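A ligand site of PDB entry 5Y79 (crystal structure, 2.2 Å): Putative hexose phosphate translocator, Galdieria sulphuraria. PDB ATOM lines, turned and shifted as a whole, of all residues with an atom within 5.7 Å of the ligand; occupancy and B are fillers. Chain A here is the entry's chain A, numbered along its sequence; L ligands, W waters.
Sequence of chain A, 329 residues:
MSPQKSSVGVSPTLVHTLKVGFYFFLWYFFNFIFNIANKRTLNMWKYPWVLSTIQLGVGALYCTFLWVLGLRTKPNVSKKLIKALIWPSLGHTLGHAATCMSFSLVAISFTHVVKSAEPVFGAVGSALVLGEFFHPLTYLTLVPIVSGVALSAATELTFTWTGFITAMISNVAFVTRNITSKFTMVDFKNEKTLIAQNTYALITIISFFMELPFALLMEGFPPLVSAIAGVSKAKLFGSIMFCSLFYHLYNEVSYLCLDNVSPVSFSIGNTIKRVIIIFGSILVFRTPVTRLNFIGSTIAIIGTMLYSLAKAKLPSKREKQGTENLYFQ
The guanidinium group of Arg 274 is in salt-bridge range of an oxygen (O7) of the ligand, at 2.8 Å. O7 of the ligand is in salt-bridge range of NZ of Lys 273, at 2.8 Å. The side-chain amino group (NZ) of Lys 115 lies within salt-bridge range of an oxygen (O5) of the ligand (2.9 Å). An oxygen (O6) of the ligand lies within hydrogen-bond range of the side-chain hydroxyl (OH) of Tyr 250. ND1 of His 96 is in hydrogen-bond range of O1 of the ligand.
The side-chain amide oxygen (OD1) of Asn 270 sits close to the guanidinium group (NH1) of Arg 274 (3.4 Å). A ring nitrogen (ND1) of His 112 lies within hydrogen-bond range of the guanidinium group of Arg 274, at 3.1 Å. A ring nitrogen (NE2) of His 96 sits close to the side-chain amide oxygen (OE1) of Gln 55 (3.4 Å). The backbone carbonyl oxygen (O) of Gly 95 is in hydrogen-bond range of the side-chain hydroxyl (OG1) of Thr 99 (2.6 Å). The backbone carbonyl oxygen (O) of Lys 115 lies within hydrogen-bond range of the guanidinium group (NE) of Arg 274 (3.4 Å). NH1 of Arg 274 is in salt-bridge range of OE2 of Glu 118, 3.1 Å away. ND2 of Asn 251 sits at hydrogen-bond distance from O of Tyr 247 (2.7 Å). The side-chain hydroxyl (OH) of Tyr 250 lies close to the side-chain amide nitrogen (ND2) of Asn 251 (3.5 Å).
Water W3 lies within hydrogen-bond range of an oxygen (O2) of the ligand (2.7 Å), the side-chain amide oxygen (OE1) of Gln 55 (3.0 Å), the side-chain amide nitrogen (ND2) of Asn 38 (3.3 Å) and the side-chain sulfur (SG) of Cys 100 (3.4 Å). Water W5 bridges O1 of the ligand and OH of Tyr 247. Water W2 lies within hydrogen-bond range of O7 of the ligand (2.8 Å), ND2 of Asn 31 (2.9 Å) and ND2 of Asn 35 (3.0 Å). Water W1 lies within hydrogen-bond range of NZ of Lys 273 (2.7 Å), O6 of the ligand (2.8 Å) and OD1 of Asn 270 (3.4 Å). Water W6 lies within hydrogen-bond range of O5 of the ligand (2.9 Å) and NH1 of Arg 177 (3.1 Å). Water W4 lies within hydrogen-bond range of the side-chain amide oxygen (OD1) of Asn 251 (2.6 Å), an oxygen (O6) of the ligand (3.0 Å) and the guanidinium group (NH2) of Arg 177 (3.0 Å).
CE2 of Phe 34 touches O3 of the ligand, at 3.1 Å. Thr 99 touches the ligand (CG2 to C2, 3.5 Å). CE2 of Phe 103 touches O3 of the ligand, at 3.6 Å. Phe 174 touches the ligand. Tyr 247 touches the ligand (CE1 to O2, 3.7 Å). Of the 22 residues printed, 10 come within 4 Å of the ligand.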
ATOM      1  N   ASN A  31     -14.516 -30.719  13.337  1.00  0.00           N
ATOM      2  CA  ASN A  31     -15.947 -30.622  13.103  1.00  0.00           C
ATOM      3  C   ASN A  31     -16.353 -31.376  11.835  1.00  0.00           C
ATOM      4  O   ASN A  31     -17.438 -31.959  11.772  1.00  0.00           O
ATOM      5  CB  ASN A  31     -16.372 -29.153  13.019  1.00  0.00           C
ATOM      6  CG  ASN A  31     -17.856 -28.993  12.810  1.00  0.00           C
ATOM      7  OD1 ASN A  31     -18.343 -28.918  11.672  1.00  0.00           O
ATOM      8  ND2 ASN A  31     -18.600 -28.934  13.915  1.00  0.00           N
ATOM      9  N   PHE A  34     -16.302 -34.978  12.705  1.00  0.00           N
ATOM     10  CA  PHE A  34     -17.487 -35.257  13.511  1.00  0.00           C
ATOM     11  C   PHE A  34     -18.738 -35.371  12.639  1.00  0.00           C
ATOM     12  O   PHE A  34     -19.507 -36.322  12.777  1.00  0.00           O
ATOM     13  CB  PHE A  34     -17.686 -34.167  14.562  1.00  0.00           C
ATOM     14  CG  PHE A  34     -19.108 -34.062  15.048  1.00  0.00           C
ATOM     15  CD1 PHE A  34     -19.626 -35.002  15.929  1.00  0.00           C
ATOM     16  CD2 PHE A  34     -19.938 -33.055  14.589  1.00  0.00           C
ATOM     17  CE1 PHE A  34     -20.933 -34.923  16.357  1.00  0.00           C
ATOM     18  CE2 PHE A  34     -21.254 -32.974  15.022  1.00  0.00           C
ATOM     19  CZ  PHE A  34     -21.744 -33.907  15.910  1.00  0.00           C
ATOM     20  N   ASN A  35     -18.970 -34.385  11.767  1.00  0.00           N
ATOM     21  CA  ASN A  35     -20.216 -34.344  11.018  1.00  0.00           C
ATOM     22  C   ASN A  35     -20.407 -35.602  10.172  1.00  0.00           C
ATOM     23  O   ASN A  35     -21.499 -36.170  10.134  1.00  0.00           O
ATOM     24  CB  ASN A  35     -20.278 -33.091  10.141  1.00  0.00           C
ATOM     25  CG  ASN A  35     -20.966 -31.927  10.823  1.00  0.00           C
ATOM     26  OD1 ASN A  35     -22.197 -31.841  10.833  1.00  0.00           O
ATOM     27  ND2 ASN A  35     -20.180 -31.015  11.395  1.00  0.00           N
ATOM     28  N   ASN A  38     -20.983 -38.536  12.586  1.00  0.00           N
ATOM     29  CA  ASN A  38     -22.256 -38.381  13.276  1.00  0.00           C
ATOM     30  C   ASN A  38     -23.428 -38.744  12.376  1.00  0.00           C
ATOM     31  O   ASN A  38     -24.375 -39.422  12.811  1.00  0.00           O
ATOM     32  CB  ASN A  38     -22.400 -36.946  13.789  1.00  0.00           C
ATOM     33  CG  ASN A  38     -23.643 -36.756  14.635  1.00  0.00           C
ATOM     34  OD1 ASN A  38     -23.789 -37.376  15.684  1.00  0.00           O
ATOM     35  ND2 ASN A  38     -24.533 -35.887  14.186  1.00  0.00           N
ATOM     36  N   GLN A  55     -22.915 -37.986  23.518  1.00  0.00           N
ATOM     37  CA  GLN A  55     -21.802 -37.147  23.093  1.00  0.00           C
ATOM     38  C   GLN A  55     -21.375 -36.191  24.203  1.00  0.00           C
ATOM     39  O   GLN A  55     -20.183 -35.965  24.408  1.00  0.00           O
ATOM     40  CB  GLN A  55     -22.174 -36.392  21.818  1.00  0.00           C
ATOM     41  CG  GLN A  55     -22.268 -37.290  20.597  1.00  0.00           C
ATOM     42  CD  GLN A  55     -23.022 -36.654  19.432  1.00  0.00           C
ATOM     43  OE1 GLN A  55     -23.683 -35.628  19.595  1.00  0.00           O
ATOM     44  NE2 GLN A  55     -22.936 -37.258  18.259  1.00  0.00           N
ATOM     45  N   GLY A  95     -29.340 -26.114  21.742  1.00  0.00           N
ATOM     46  CA  GLY A  95     -28.790 -26.127  20.390  1.00  0.00           C
ATOM     47  C   GLY A  95     -28.266 -27.491  19.991  1.00  0.00           C
ATOM     48  O   GLY A  95     -28.401 -27.893  18.835  1.00  0.00           O
ATOM     49  N   HIS A  96     -27.674 -28.214  20.942  1.00  0.00           N
ATOM     50  CA  HIS A  96     -27.139 -29.536  20.660  1.00  0.00           C
ATOM     51  C   HIS A  96     -28.255 -30.512  20.321  1.00  0.00           C
ATOM     52  O   HIS A  96     -28.190 -31.220  19.311  1.00  0.00           O
ATOM     53  CB  HIS A  96     -26.333 -30.034  21.868  1.00  0.00           C
ATOM     54  CG  HIS A  96     -25.703 -31.374  21.668  1.00  0.00           C
ATOM     55  ND1 HIS A  96     -25.041 -31.724  20.508  1.00  0.00           N
ATOM     56  CD2 HIS A  96     -25.618 -32.446  22.489  1.00  0.00           C
ATOM     57  CE1 HIS A  96     -24.585 -32.962  20.620  1.00  0.00           C
ATOM     58  NE2 HIS A  96     -24.919 -33.419  21.813  1.00  0.00           N
ATOM     59  N   ALA A  97     -29.297 -30.564  21.153  1.00  0.00           N
ATOM     60  CA  ALA A  97     -30.407 -31.473  20.913  1.00  0.00           C
ATOM     61  C   ALA A  97     -31.170 -31.097  19.639  1.00  0.00           C
ATOM     62  O   ALA A  97     -31.600 -31.967  18.873  1.00  0.00           O
ATOM     63  CB  ALA A  97     -31.339 -31.510  22.115  1.00  0.00           C
ATOM     64  N   THR A  99     -30.002 -29.456  16.929  1.00  0.00           N
ATOM     65  CA  THR A  99     -29.219 -29.713  15.718  1.00  0.00           C
ATOM     66  C   THR A  99     -29.120 -31.204  15.436  1.00  0.00           C
ATOM     67  O   THR A  99     -29.203 -31.633  14.282  1.00  0.00           O
ATOM     68  CB  THR A  99     -27.837 -29.095  15.834  1.00  0.00           C
ATOM     69  OG1 THR A  99     -27.957 -27.726  16.240  1.00  0.00           O
ATOM     70  CG2 THR A  99     -27.130 -29.143  14.493  1.00  0.00           C
ATOM     71  N   CYS A 100     -28.956 -32.016  16.483  1.00  0.00           N
ATOM     72  CA  CYS A 100     -28.929 -33.470  16.291  1.00  0.00           C
ATOM     73  C   CYS A 100     -30.263 -33.971  15.743  1.00  0.00           C
ATOM     74  O   CYS A 100     -30.280 -34.836  14.865  1.00  0.00           O
ATOM     75  CB  CYS A 100     -28.576 -34.171  17.597  1.00  0.00           C
ATOM     76  SG  CYS A 100     -28.155 -35.910  17.384  1.00  0.00           S
ATOM     77  N   PHE A 103     -30.163 -33.093  12.154  1.00  0.00           N
ATOM     78  CA  PHE A 103     -29.287 -34.060  11.486  1.00  0.00           C
ATOM     79  C   PHE A 103     -30.008 -35.373  11.242  1.00  0.00           C
ATOM     80  O   PHE A 103     -29.797 -36.009  10.195  1.00  0.00           O
ATOM     81  CB  PHE A 103     -28.035 -34.309  12.337  1.00  0.00           C
ATOM     82  CG  PHE A 103     -27.029 -33.181  12.298  1.00  0.00           C
ATOM     83  CD1 PHE A 103     -27.045 -32.237  11.284  1.00  0.00           C
ATOM     84  CD2 PHE A 103     -26.056 -33.092  13.286  1.00  0.00           C
ATOM     85  CE1 PHE A 103     -26.109 -31.207  11.261  1.00  0.00           C
ATOM     86  CE2 PHE A 103     -25.120 -32.063  13.264  1.00  0.00           C
ATOM     87  CZ  PHE A 103     -25.149 -31.124  12.249  1.00  0.00           C
ATOM     88  N   HIS A 112     -26.897 -27.296   7.907  1.00  0.00           N
ATOM     89  CA  HIS A 112     -25.848 -26.291   8.008  1.00  0.00           C
ATOM     90  C   HIS A 112     -26.166 -25.042   7.189  1.00  0.00           C
ATOM     91  O   HIS A 112     -25.674 -23.953   7.528  1.00  0.00           O
ATOM     92  CB  HIS A 112     -24.504 -26.892   7.586  1.00  0.00           C
ATOM     93  CG  HIS A 112     -23.902 -27.802   8.617  1.00  0.00           C
ATOM     94  ND1 HIS A 112     -23.338 -27.330   9.779  1.00  0.00           N
ATOM     95  CD2 HIS A 112     -23.772 -29.145   8.649  1.00  0.00           C
ATOM     96  CE1 HIS A 112     -22.887 -28.348  10.488  1.00  0.00           C
ATOM     97  NE2 HIS A 112     -23.136 -29.466   9.827  1.00  0.00           N
ATOM     98  N   LYS A 115     -28.266 -23.125   9.543  1.00  0.00           N
ATOM     99  CA  LYS A 115     -27.432 -22.594  10.604  1.00  0.00           C
ATOM    100  C   LYS A 115     -26.418 -21.579  10.108  1.00  0.00           C
ATOM    101  O   LYS A 115     -25.788 -20.899  10.924  1.00  0.00           O
ATOM    102  CB  LYS A 115     -26.739 -23.743  11.353  1.00  0.00           C
ATOM    103  CG  LYS A 115     -27.718 -24.585  12.181  1.00  0.00           C
ATOM    104  CD  LYS A 115     -27.137 -25.926  12.611  1.00  0.00           C
ATOM    105  CE  LYS A 115     -25.924 -25.763  13.520  1.00  0.00           C
ATOM    106  NZ  LYS A 115     -26.236 -25.015  14.771  1.00  0.00           N
ATOM    107  N   GLU A 118     -26.606 -17.948  11.358  1.00  0.00           N
ATOM    108  CA  GLU A 118     -26.260 -17.678  12.743  1.00  0.00           C
ATOM    109  C   GLU A 118     -25.687 -16.282  12.995  1.00  0.00           C
ATOM    110  O   GLU A 118     -26.022 -15.698  14.046  1.00  0.00           O
ATOM    111  CB  GLU A 118     -25.278 -18.756  13.240  1.00  0.00           C
ATOM    112  CG  GLU A 118     -25.137 -18.847  14.741  1.00  0.00           C
ATOM    113  CD  GLU A 118     -23.984 -19.742  15.158  1.00  0.00           C
ATOM    114  OE1 GLU A 118     -22.982 -19.218  15.695  1.00  0.00           O
ATOM    115  OE2 GLU A 118     -24.071 -20.973  14.936  1.00  0.00           O
ATOM    116  N   PHE A 174     -27.546 -21.383  20.367  1.00  0.00           N
ATOM    117  CA  PHE A 174     -26.087 -21.291  20.370  1.00  0.00           C
ATOM    118  C   PHE A 174     -25.615 -19.847  20.513  1.00  0.00           C
ATOM    119  O   PHE A 174     -24.550 -19.603  21.094  1.00  0.00           O
ATOM    120  CB  PHE A 174     -25.520 -21.916  19.094  1.00  0.00           C
ATOM    121  CG  PHE A 174     -25.484 -23.425  19.128  1.00  0.00           C
ATOM    122  CD1 PHE A 174     -24.987 -24.096  20.228  1.00  0.00           C
ATOM    123  CD2 PHE A 174     -25.960 -24.163  18.051  1.00  0.00           C
ATOM    124  CE1 PHE A 174     -24.956 -25.480  20.265  1.00  0.00           C
ATOM    125  CE2 PHE A 174     -25.929 -25.546  18.088  1.00  0.00           C
ATOM    126  CZ  PHE A 174     -25.424 -26.201  19.197  1.00  0.00           C
ATOM    127  N   ARG A 177     -25.733 -19.075  24.113  1.00  0.00           N
ATOM    128  CA  ARG A 177     -24.583 -19.765  24.705  1.00  0.00           C
ATOM    129  C   ARG A 177     -23.304 -18.963  24.490  1.00  0.00           C
ATOM    130  O   ARG A 177     -22.547 -18.717  25.434  1.00  0.00           O
ATOM    131  CB  ARG A 177     -24.439 -21.169  24.112  1.00  0.00           C
ATOM    132  CG  ARG A 177     -23.216 -21.915  24.626  1.00  0.00           C
ATOM    133  CD  ARG A 177     -22.797 -23.056  23.693  1.00  0.00           C
ATOM    134  NE  ARG A 177     -22.133 -22.569  22.486  1.00  0.00           N
ATOM    135  CZ  ARG A 177     -21.631 -23.356  21.538  1.00  0.00           C
ATOM    136  NH1 ARG A 177     -21.034 -22.827  20.473  1.00  0.00           N
ATOM    137  NH2 ARG A 177     -21.742 -24.671  21.647  1.00  0.00           N
ATOM    138  N   TYR A 247     -16.952 -34.907  18.479  1.00  0.00           N
ATOM    139  CA  TYR A 247     -17.887 -33.882  18.914  1.00  0.00           C
ATOM    140  C   TYR A 247     -17.279 -33.027  20.019  1.00  0.00           C
ATOM    141  O   TYR A 247     -17.354 -31.798  19.987  1.00  0.00           O
ATOM    142  CB  TYR A 247     -19.190 -34.503  19.410  1.00  0.00           C
ATOM    143  CG  TYR A 247     -20.079 -33.495  20.126  1.00  0.00           C
ATOM    144  CD1 TYR A 247     -20.914 -32.640  19.404  1.00  0.00           C
ATOM    145  CD2 TYR A 247     -20.061 -33.375  21.515  1.00  0.00           C
ATOM    146  CE1 TYR A 247     -21.711 -31.710  20.044  1.00  0.00           C
ATOM    147  CE2 TYR A 247     -20.853 -32.437  22.158  1.00  0.00           C
ATOM    148  CZ  TYR A 247     -21.681 -31.615  21.423  1.00  0.00           C
ATOM    149  OH  TYR A 247     -22.464 -30.679  22.062  1.00  0.00           O
ATOM    150  N   TYR A 250     -14.001 -30.840  18.790  1.00  0.00           N
ATOM    151  CA  TYR A 250     -14.268 -29.633  18.001  1.00  0.00           C
ATOM    152  C   TYR A 250     -14.892 -28.540  18.866  1.00  0.00           C
ATOM    153  O   TYR A 250     -14.539 -27.371  18.735  1.00  0.00           O
ATOM    154  CB  TYR A 250     -15.139 -29.952  16.773  1.00  0.00           C
ATOM    155  CG  TYR A 250     -16.650 -29.756  16.882  1.00  0.00           C
ATOM    156  CD1 TYR A 250     -17.206 -28.472  16.913  1.00  0.00           C
ATOM    157  CD2 TYR A 250     -17.513 -30.840  16.891  1.00  0.00           C
ATOM    158  CE1 TYR A 250     -18.574 -28.296  16.997  1.00  0.00           C
ATOM    159  CE2 TYR A 250     -18.888 -30.666  16.962  1.00  0.00           C
ATOM    160  CZ  TYR A 250     -19.410 -29.387  17.018  1.00  0.00           C
ATOM    161  OH  TYR A 250     -20.772 -29.207  17.089  1.00  0.00           O
ATOM    162  N   ASN A 251     -15.816 -28.905  19.751  1.00  0.00           N
ATOM    163  CA  ASN A 251     -16.410 -27.908  20.627  1.00  0.00           C
ATOM    164  C   ASN A 251     -15.378 -27.334  21.587  1.00  0.00           C
ATOM    165  O   ASN A 251     -15.350 -26.127  21.838  1.00  0.00           O
ATOM    166  CB  ASN A 251     -17.575 -28.508  21.411  1.00  0.00           C
ATOM    167  CG  ASN A 251     -18.844 -28.570  20.596  1.00  0.00           C
ATOM    168  OD1 ASN A 251     -19.522 -27.555  20.411  1.00  0.00           O
ATOM    169  ND2 ASN A 251     -19.186 -29.758  20.120  1.00  0.00           N
ATOM    170  N   ASN A 270     -18.199 -19.559  12.309  1.00  0.00           N
ATOM    171  CA  ASN A 270     -19.040 -20.737  12.153  1.00  0.00           C
ATOM    172  C   ASN A 270     -19.589 -20.844  10.725  1.00  0.00           C
ATOM    173  O   ASN A 270     -19.684 -21.942  10.179  1.00  0.00           O
ATOM    174  CB  ASN A 270     -20.184 -20.708  13.156  1.00  0.00           C
ATOM    175  CG  ASN A 270     -20.143 -21.887  14.120  1.00  0.00           C
ATOM    176  OD1 ASN A 270     -19.625 -22.958  13.806  1.00  0.00           O
ATOM    177  ND2 ASN A 270     -20.696 -21.685  15.314  1.00  0.00           N
ATOM    178  N   LYS A 273     -16.981 -22.169   8.576  1.00  0.00           N
ATOM    179  CA  LYS A 273     -16.939 -23.608   8.838  1.00  0.00           C
ATOM    180  C   LYS A 273     -18.013 -24.341   8.046  1.00  0.00           C
ATOM    181  O   LYS A 273     -17.756 -25.424   7.493  1.00  0.00           O
ATOM    182  CB  LYS A 273     -17.109 -23.866  10.337  1.00  0.00           C
ATOM    183  CG  LYS A 273     -16.982 -25.338  10.739  1.00  0.00           C
ATOM    184  CD  LYS A 273     -17.358 -25.544  12.193  1.00  0.00           C
ATOM    185  CE  LYS A 273     -18.873 -25.668  12.365  1.00  0.00           C
ATOM    186  NZ  LYS A 273     -19.249 -25.789  13.803  1.00  0.00           N
ATOM    187  N   ARG A 274     -19.211 -23.764   7.952  1.00  0.00           N
ATOM    188  CA  ARG A 274     -20.325 -24.499   7.377  1.00  0.00           C
ATOM    189  C   ARG A 274     -20.214 -24.626   5.863  1.00  0.00           C
ATOM    190  O   ARG A 274     -20.672 -25.619   5.299  1.00  0.00           O
ATOM    191  CB  ARG A 274     -21.642 -23.839   7.781  1.00  0.00           C
ATOM    192  CG  ARG A 274     -21.877 -23.962   9.273  1.00  0.00           C
ATOM    193  CD  ARG A 274     -23.199 -23.373   9.743  1.00  0.00           C
ATOM    194  NE  ARG A 274     -23.102 -22.992  11.152  1.00  0.00           N
ATOM    195  CZ  ARG A 274     -23.052 -23.844  12.171  1.00  0.00           C
ATOM    196  NH1 ARG A 274     -22.964 -23.393  13.417  1.00  0.00           N
ATOM    197  NH2 ARG A 274     -23.078 -25.155  11.947  1.00  0.00           N
HETATM  198  C1  LIG L   1     -24.432 -30.716  17.441  1.00  0.00           C
HETATM  199  O1  LIG L   1     -24.794 -30.125  18.480  1.00  0.00           O
HETATM  200  O2  LIG L   1     -24.323 -31.966  17.368  1.00  0.00           O
HETATM  201  C2  LIG L   1     -24.126 -29.905  16.219  1.00  0.00           C
HETATM  202  O3  LIG L   1     -22.933 -30.418  15.618  1.00  0.00           O
HETATM  203  C3  LIG L   1     -23.910 -28.451  16.597  1.00  0.00           C
HETATM  204  O4  LIG L   1     -23.638 -27.716  15.409  1.00  0.00           O
HETATM  205  P1  LIG L   1     -22.590 -26.494  15.411  1.00  0.00           P
HETATM  206  O5  LIG L   1     -23.444 -25.260  15.598  1.00  0.00           O
HETATM  207  O6  LIG L   1     -21.679 -26.786  16.579  1.00  0.00           O
HETATM  208  O7  LIG L   1     -21.936 -26.611  14.063  1.00  0.00           O
HETATM  209  O   HOH W   1     -19.399 -25.125  16.388  1.00  0.00           O
HETATM  210  O   HOH W   2     -21.430 -29.269  13.539  1.00  0.00           O
HETATM  211  O   HOH W   3     -25.099 -34.498  17.144  1.00  0.00           O
HETATM  212  O   HOH W   4     -21.858 -26.821  19.551  1.00  0.00           O
HETATM  213  O   HOH W   5     -23.377 -28.618  20.293  1.00  0.00           O
HETATM  214  O   HOH W   6     -22.477 -23.649  17.808  1.00  0.00           O
